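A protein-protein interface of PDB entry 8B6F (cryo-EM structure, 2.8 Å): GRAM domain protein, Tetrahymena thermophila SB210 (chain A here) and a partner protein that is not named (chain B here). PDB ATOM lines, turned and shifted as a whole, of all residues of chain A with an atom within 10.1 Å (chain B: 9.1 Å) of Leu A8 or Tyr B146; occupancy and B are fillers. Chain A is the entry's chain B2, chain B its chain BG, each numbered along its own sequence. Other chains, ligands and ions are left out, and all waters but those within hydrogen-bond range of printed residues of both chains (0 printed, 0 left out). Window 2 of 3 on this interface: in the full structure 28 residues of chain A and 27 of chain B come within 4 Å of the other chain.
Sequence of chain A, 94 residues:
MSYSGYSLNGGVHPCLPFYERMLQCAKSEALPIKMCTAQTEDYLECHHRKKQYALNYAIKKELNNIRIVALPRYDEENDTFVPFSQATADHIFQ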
ATOM      1  N   SER A   4     -40.250 -25.492 -25.700  1.00  0.00           N
ATOM      2  CA  SER A   4     -40.049 -26.171 -26.976  1.00  0.00           C
ATOM      3  C   SER A   4     -39.792 -27.659 -26.782  1.00  0.00           C
ATOM      4  O   SER A   4     -40.272 -28.486 -27.565  1.00  0.00           O
ATOM      5  CB  SER A   4     -38.891 -25.526 -27.728  1.00  0.00           C
ATOM      6  OG  SER A   4     -37.703 -25.656 -26.979  1.00  0.00           O
ATOM      7  N   GLY A   5     -39.035 -28.019 -25.752  1.00  0.00           N
ATOM      8  CA  GLY A   5     -38.697 -29.405 -25.507  1.00  0.00           C
ATOM      9  C   GLY A   5     -37.492 -29.919 -26.261  1.00  0.00           C
ATOM     10  O   GLY A   5     -37.281 -31.136 -26.294  1.00  0.00           O
ATOM     11  N   TYR A   6     -36.700 -29.042 -26.869  1.00  0.00           N
ATOM     12  CA  TYR A   6     -35.492 -29.429 -27.579  1.00  0.00           C
ATOM     13  C   TYR A   6     -34.258 -29.174 -26.719  1.00  0.00           C
ATOM     14  O   TYR A   6     -34.276 -28.373 -25.783  1.00  0.00           O
ATOM     15  CB  TYR A   6     -35.364 -28.659 -28.894  1.00  0.00           C
ATOM     16  CG  TYR A   6     -36.414 -28.999 -29.919  1.00  0.00           C
ATOM     17  CD1 TYR A   6     -36.305 -30.141 -30.701  1.00  0.00           C
ATOM     18  CD2 TYR A   6     -37.507 -28.170 -30.121  1.00  0.00           C
ATOM     19  CE1 TYR A   6     -37.260 -30.452 -31.646  1.00  0.00           C
ATOM     20  CE2 TYR A   6     -38.467 -28.472 -31.063  1.00  0.00           C
ATOM     21  CZ  TYR A   6     -38.339 -29.613 -31.823  1.00  0.00           C
ATOM     22  OH  TYR A   6     -39.294 -29.915 -32.762  1.00  0.00           O
ATOM     23  N   SER A   7     -33.177 -29.872 -27.056  1.00  0.00           N
ATOM     24  CA  SER A   7     -31.894 -29.667 -26.404  1.00  0.00           C
ATOM     25  C   SER A   7     -31.086 -28.649 -27.208  1.00  0.00           C
ATOM     26  O   SER A   7     -31.589 -28.030 -28.147  1.00  0.00           O
ATOM     27  CB  SER A   7     -31.157 -30.994 -26.249  1.00  0.00           C
ATOM     28  OG  SER A   7     -30.844 -31.557 -27.510  1.00  0.00           O
ATOM     29  N   LEU A   8     -29.819 -28.464 -26.845  1.00  0.00           N
ATOM     30  CA  LEU A   8     -28.963 -27.513 -27.542  1.00  0.00           C
ATOM     31  C   LEU A   8     -28.314 -28.097 -28.789  1.00  0.00           C
ATOM     32  O   LEU A   8     -27.598 -27.373 -29.488  1.00  0.00           O
ATOM     33  CB  LEU A   8     -27.877 -26.993 -26.596  1.00  0.00           C
ATOM     34  CG  LEU A   8     -28.363 -26.262 -25.339  1.00  0.00           C
ATOM     35  CD1 LEU A   8     -27.202 -25.615 -24.604  1.00  0.00           C
ATOM     36  CD2 LEU A   8     -29.445 -25.249 -25.651  1.00  0.00           C
ATOM     37  N   ASN A   9     -28.535 -29.379 -29.080  1.00  0.00           N
ATOM     38  CA  ASN A   9     -28.062 -29.997 -30.313  1.00  0.00           C
ATOM     39  C   ASN A   9     -29.216 -30.553 -31.137  1.00  0.00           C
ATOM     40  O   ASN A   9     -29.014 -31.459 -31.951  1.00  0.00           O
ATOM     41  CB  ASN A   9     -27.049 -31.102 -30.009  1.00  0.00           C
ATOM     42  CG  ASN A   9     -27.654 -32.249 -29.231  1.00  0.00           C
ATOM     43  OD1 ASN A   9     -28.632 -32.075 -28.506  1.00  0.00           O
ATOM     44  ND2 ASN A   9     -27.073 -33.432 -29.377  1.00  0.00           N
ATOM     45  N   GLY A  10     -30.424 -30.030 -30.940  1.00  0.00           N
ATOM     46  CA  GLY A  10     -31.593 -30.522 -31.631  1.00  0.00           C
ATOM     47  C   GLY A  10     -32.233 -31.742 -31.011  1.00  0.00           C
ATOM     48  O   GLY A  10     -33.253 -32.214 -31.528  1.00  0.00           O
ATOM     49  N   GLY A  11     -31.678 -32.266 -29.922  1.00  0.00           N
ATOM     50  CA  GLY A  11     -32.227 -33.434 -29.260  1.00  0.00           C
ATOM     51  C   GLY A  11     -33.463 -33.101 -28.455  1.00  0.00           C
ATOM     52  O   GLY A  11     -34.243 -32.209 -28.805  1.00  0.00           O
ATOM     53  N   VAL A  12     -33.647 -33.826 -27.356  1.00  0.00           N
ATOM     54  CA  VAL A  12     -34.802 -33.664 -26.480  1.00  0.00           C
ATOM     55  C   VAL A  12     -34.345 -33.034 -25.175  1.00  0.00           C
ATOM     56  O   VAL A  12     -33.329 -33.439 -24.599  1.00  0.00           O
ATOM     57  CB  VAL A  12     -35.515 -35.006 -26.235  1.00  0.00           C
ATOM     58  CG1 VAL A  12     -36.411 -34.942 -25.005  1.00  0.00           C
ATOM     59  CG2 VAL A  12     -36.338 -35.374 -27.449  1.00  0.00           C
ATOM     60  N   HIS A  13     -35.101 -32.043 -24.715  1.00  0.00           N
ATOM     61  CA  HIS A  13     -34.772 -31.363 -23.476  1.00  0.00           C
ATOM     62  C   HIS A  13     -34.798 -32.363 -22.323  1.00  0.00           C
ATOM     63  O   HIS A  13     -35.714 -33.190 -22.241  1.00  0.00           O
ATOM     64  CB  HIS A  13     -35.769 -30.231 -23.222  1.00  0.00           C
ATOM     65  CG  HIS A  13     -35.316 -29.243 -22.196  1.00  0.00           C
ATOM     66  ND1 HIS A  13     -35.782 -29.254 -20.899  1.00  0.00           N
ATOM     67  CD2 HIS A  13     -34.444 -28.212 -22.274  1.00  0.00           C
ATOM     68  CE1 HIS A  13     -35.213 -28.274 -20.221  1.00  0.00           C
ATOM     69  NE2 HIS A  13     -34.398 -27.626 -21.032  1.00  0.00           N
ATOM     70  N   PRO A  14     -33.819 -32.323 -21.415  1.00  0.00           N
ATOM     71  CA  PRO A  14     -33.798 -33.313 -20.325  1.00  0.00           C
ATOM     72  C   PRO A  14     -35.010 -33.252 -19.413  1.00  0.00           C
ATOM     73  O   PRO A  14     -35.322 -34.256 -18.763  1.00  0.00           O
ATOM     74  CB  PRO A  14     -32.505 -32.973 -19.569  1.00  0.00           C
ATOM     75  CG  PRO A  14     -32.228 -31.555 -19.907  1.00  0.00           C
ATOM     76  CD  PRO A  14     -32.696 -31.375 -21.314  1.00  0.00           C
ATOM     77  N   ARG A  49     -32.462 -27.462 -10.019  1.00  0.00           N
ATOM     78  CA  ARG A  49     -31.412 -28.224  -9.348  1.00  0.00           C
ATOM     79  C   ARG A  49     -31.073 -27.635  -7.983  1.00  0.00           C
ATOM     80  O   ARG A  49     -29.921 -27.680  -7.548  1.00  0.00           O
ATOM     81  CB  ARG A  49     -30.154 -28.327 -10.217  1.00  0.00           C
ATOM     82  CG  ARG A  49     -30.374 -29.097 -11.507  1.00  0.00           C
ATOM     83  CD  ARG A  49     -29.504 -28.575 -12.634  1.00  0.00           C
ATOM     84  NE  ARG A  49     -29.981 -27.297 -13.146  1.00  0.00           N
ATOM     85  CZ  ARG A  49     -29.406 -26.624 -14.132  1.00  0.00           C
ATOM     86  NH1 ARG A  49     -28.321 -27.076 -14.738  1.00  0.00           N
ATOM     87  NH2 ARG A  49     -29.932 -25.468 -14.521  1.00  0.00           N
ATOM     88  N   ARG B 143     -24.100 -26.600 -16.583  1.00  0.00           N
ATOM     89  CA  ARG B 143     -24.492 -26.080 -17.883  1.00  0.00           C
ATOM     90  C   ARG B 143     -24.501 -27.233 -18.871  1.00  0.00           C
ATOM     91  O   ARG B 143     -23.951 -28.305 -18.609  1.00  0.00           O
ATOM     92  CB  ARG B 143     -23.544 -24.975 -18.360  1.00  0.00           C
ATOM     93  CG  ARG B 143     -22.126 -25.461 -18.631  1.00  0.00           C
ATOM     94  CD  ARG B 143     -21.254 -24.350 -19.169  1.00  0.00           C
ATOM     95  NE  ARG B 143     -21.743 -23.836 -20.442  1.00  0.00           N
ATOM     96  CZ  ARG B 143     -21.410 -24.322 -21.629  1.00  0.00           C
ATOM     97  NH1 ARG B 143     -20.588 -25.351 -21.750  1.00  0.00           N
ATOM     98  NH2 ARG B 143     -21.914 -23.763 -22.723  1.00  0.00           N
ATOM     99  N   TYR B 144     -25.130 -27.001 -20.018  1.00  0.00           N
ATOM    100  CA  TYR B 144     -25.248 -27.996 -21.073  1.00  0.00           C
ATOM    101  C   TYR B 144     -24.379 -27.588 -22.254  1.00  0.00           C
ATOM    102  O   TYR B 144     -24.389 -26.425 -22.667  1.00  0.00           O
ATOM    103  CB  TYR B 144     -26.704 -28.155 -21.512  1.00  0.00           C
ATOM    104  CG  TYR B 144     -27.621 -28.573 -20.389  1.00  0.00           C
ATOM    105  CD1 TYR B 144     -28.129 -27.638 -19.498  1.00  0.00           C
ATOM    106  CD2 TYR B 144     -27.969 -29.904 -20.213  1.00  0.00           C
ATOM    107  CE1 TYR B 144     -28.964 -28.014 -18.469  1.00  0.00           C
ATOM    108  CE2 TYR B 144     -28.803 -30.290 -19.187  1.00  0.00           C
ATOM    109  CZ  TYR B 144     -29.297 -29.340 -18.318  1.00  0.00           C
ATOM    110  OH  TYR B 144     -30.127 -29.722 -17.292  1.00  0.00           O
ATOM    111  N   ALA B 145     -23.625 -28.545 -22.786  1.00  0.00           N
ATOM    112  CA  ALA B 145     -22.749 -28.265 -23.913  1.00  0.00           C
ATOM    113  C   ALA B 145     -23.564 -27.898 -25.146  1.00  0.00           C
ATOM    114  O   ALA B 145     -24.604 -28.501 -25.426  1.00  0.00           O
ATOM    115  CB  ALA B 145     -21.866 -29.474 -24.214  1.00  0.00           C
ATOM    116  N   TYR B 146     -23.088 -26.897 -25.882  1.00  0.00           N
ATOM    117  CA  TYR B 146     -23.727 -26.456 -27.115  1.00  0.00           C
ATOM    118  C   TYR B 146     -22.831 -26.631 -28.330  1.00  0.00           C
ATOM    119  O   TYR B 146     -23.250 -27.241 -29.320  1.00  0.00           O
ATOM    120  CB  TYR B 146     -24.153 -24.988 -26.987  1.00  0.00           C
ATOM    121  CG  TYR B 146     -24.492 -24.336 -28.306  1.00  0.00           C
ATOM    122  CD1 TYR B 146     -25.688 -24.610 -28.953  1.00  0.00           C
ATOM    123  CD2 TYR B 146     -23.620 -23.435 -28.898  1.00  0.00           C
ATOM    124  CE1 TYR B 146     -25.999 -24.012 -30.157  1.00  0.00           C
ATOM    125  CE2 TYR B 146     -23.923 -22.833 -30.100  1.00  0.00           C
ATOM    126  CZ  TYR B 146     -25.114 -23.123 -30.723  1.00  0.00           C
ATOM    127  OH  TYR B 146     -25.419 -22.524 -31.923  1.00  0.00           O
ATOM    128  N   MET B 147     -21.604 -26.123 -28.278  1.00  0.00           N
ATOM    129  CA  MET B 147     -20.733 -26.140 -29.442  1.00  0.00           C
ATOM    130  C   MET B 147     -20.368 -27.567 -29.834  1.00  0.00           C
ATOM    131  O   MET B 147     -20.328 -28.476 -29.002  1.00  0.00           O
ATOM    132  CB  MET B 147     -19.460 -25.341 -29.165  1.00  0.00           C
ATOM    133  CG  MET B 147     -19.570 -23.850 -29.444  1.00  0.00           C
ATOM    134  SD  MET B 147     -19.369 -23.472 -31.194  1.00  0.00           S
ATOM    135  CE  MET B 147     -21.071 -23.255 -31.697  1.00  0.00           C
ATOM    136  N   TYR B 148     -20.094 -27.750 -31.124  1.00  0.00           N
ATOM    137  CA  TYR B 148     -19.652 -29.033 -31.666  1.00  0.00           C
ATOM    138  C   TYR B 148     -20.655 -30.139 -31.355  1.00  0.00           C
ATOM    139  O   TYR B 148     -20.300 -31.229 -30.905  1.00  0.00           O
ATOM    140  CB  TYR B 148     -18.260 -29.393 -31.144  1.00  0.00           C
ATOM    141  CG  TYR B 148     -17.213 -28.367 -31.501  1.00  0.00           C
ATOM    142  CD1 TYR B 148     -16.678 -28.311 -32.780  1.00  0.00           C
ATOM    143  CD2 TYR B 148     -16.762 -27.453 -30.560  1.00  0.00           C
ATOM    144  CE1 TYR B 148     -15.724 -27.374 -33.113  1.00  0.00           C
ATOM    145  CE2 TYR B 148     -15.808 -26.512 -30.883  1.00  0.00           C
ATOM    146  CZ  TYR B 148     -15.293 -26.477 -32.162  1.00  0.00           C
ATOM    147  OH  TYR B 148     -14.340 -25.541 -32.489  1.00  0.00           O
ATOM    148  N   ASN B 149     -21.929 -29.849 -31.609  1.00  0.00           N
ATOM    149  CA  ASN B 149     -22.999 -30.821 -31.412  1.00  0.00           C
ATOM    150  C   ASN B 149     -23.015 -31.327 -29.971  1.00  0.00           C
ATOM    151  O   ASN B 149     -23.150 -32.525 -29.715  1.00  0.00           O
ATOM    152  CB  ASN B 149     -22.861 -31.981 -32.398  1.00  0.00           C
ATOM    153  CG  ASN B 149     -24.141 -32.768 -32.555  1.00  0.00           C
ATOM    154  OD1 ASN B 149     -24.935 -32.880 -31.623  1.00  0.00           O
ATOM    155  ND2 ASN B 149     -24.351 -33.322 -33.742  1.00  0.00           N
ATOM    156  N   SER B 150     -22.867 -30.403 -29.023  1.00  0.00           N
ATOM    157  CA  SER B 150     -22.831 -30.724 -27.599  1.00  0.00           C
ATOM    158  C   SER B 150     -21.682 -31.685 -27.294  1.00  0.00           C
ATOM    159  O   SER B 150     -21.869 -32.784 -26.770  1.00  0.00           O
ATOM    160  CB  SER B 150     -24.172 -31.305 -27.137  1.00  0.00           C
ATOM    161  OG  SER B 150     -25.200 -30.333 -27.214  1.00  0.00           O
ATOM    162  N   SER B 151     -20.477 -31.244 -27.642  1.00  0.00           N
ATOM    163  CA  SER B 151     -19.261 -31.999 -27.384  1.00  0.00           C
ATOM    164  C   SER B 151     -18.164 -31.025 -26.977  1.00  0.00           C
ATOM    165  O   SER B 151     -18.359 -29.807 -26.966  1.00  0.00           O
ATOM    166  CB  SER B 151     -18.849 -32.819 -28.608  1.00  0.00           C
ATOM    167  OG  SER B 151     -19.894 -33.678 -29.026  1.00  0.00           O
ATOM    168  N   ASN B 152     -17.001 -31.573 -26.634  1.00  0.00           N
ATOM    169  CA  ASN B 152     -15.838 -30.784 -26.243  1.00  0.00           C
ATOM    170  C   ASN B 152     -14.702 -31.069 -27.213  1.00  0.00           C
ATOM    171  O   ASN B 152     -14.224 -32.206 -27.297  1.00  0.00           O
ATOM    172  CB  ASN B 152     -15.414 -31.103 -24.810  1.00  0.00           C
ATOM    173  CG  ASN B 152     -16.423 -30.627 -23.789  1.00  0.00           C
ATOM    174  OD1 ASN B 152     -16.377 -29.482 -23.343  1.00  0.00           O
ATOM    175  ND2 ASN B 152     -17.344 -31.507 -23.413  1.00  0.00           N
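Of the 12 printed residues of chain A, 4 touch a printed residue of chain B. Hydrophobic or aromatic side chains of chain A within 4 Å of the printed part of chain B: Leu A8 and Pro A14. Along chain A the printed residues that touch a printed residue of chain B span positions 8 to 49. Printed residues of chain B that touch a printed residue of chain A: Tyr B144, Ala B145, Tyr B146, Asn B149 and Ser B150. Hydrophobic or aromatic side chains of chain B within 4 Å of the printed part of chain A: Tyr B144 and Tyr B146. Among the printed residues, 7 pairs touch across the chains.
The side-chain amide oxygen of Asn B149 lies within hydrogen-bond range of the side-chain amide nitrogen of Asn A9, 3.1 Å away.
Among the printed residues, pairs that only touch across the chains: Leu A8 with Tyr B144 (3.5 Å), Leu A8 with Ala B145 (3.8 Å), Leu A8 with Tyr B146 (3.4 Å), Asn A9 with Ser B150 (3.4 Å), Pro A14 with Tyr B144 (3.7 Å) and Arg A49 with Tyr B144 (3.9 Å).
Leu A8 touches just these residues of chain B: Tyr B144, Ala B145 and Tyr B146. Of chain A, only Leu A8 comes within 4 Å of Tyr B146. No residue of chain B comes within 4 Å of Ser A7. No residue of chain A comes within 4 Å of Met B147. Printed residues of chain A within 4 Å of Tyr B144: Leu A8 (3.5 Å), Pro A14 (3.7 Å) and Arg A49 (3.9 Å). Of the printed residues of chain A, Asn B149 touches Asn A9. Of the printed residues of chain B, Arg A49 touches Tyr B144 (3.9 Å). Of the printed residues of chain A, Ser B150 touches Asn A9. Of the printed residues of chain B, Pro A14 touches Tyr B144. Ser B151 touches none of the printed residues of chain A. Ser A4 touches none of the printed residues of chain B. The nearest printed residue of chain B that does not touch Arg A49 is Arg B143 (4.6 Å).
The side-chain amide oxygen (OD1) of Asn A9 sits close to the backbone NH (N) of Gly A11. The backbone carbonyl oxygen (O) of Ala B145 lies within hydrogen-bond range of the side-chain hydroxyl (OG) of Ser B150 (2.6 Å). OG of Ser A7 is in hydrogen-bond range of OD1 of Asn A9.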
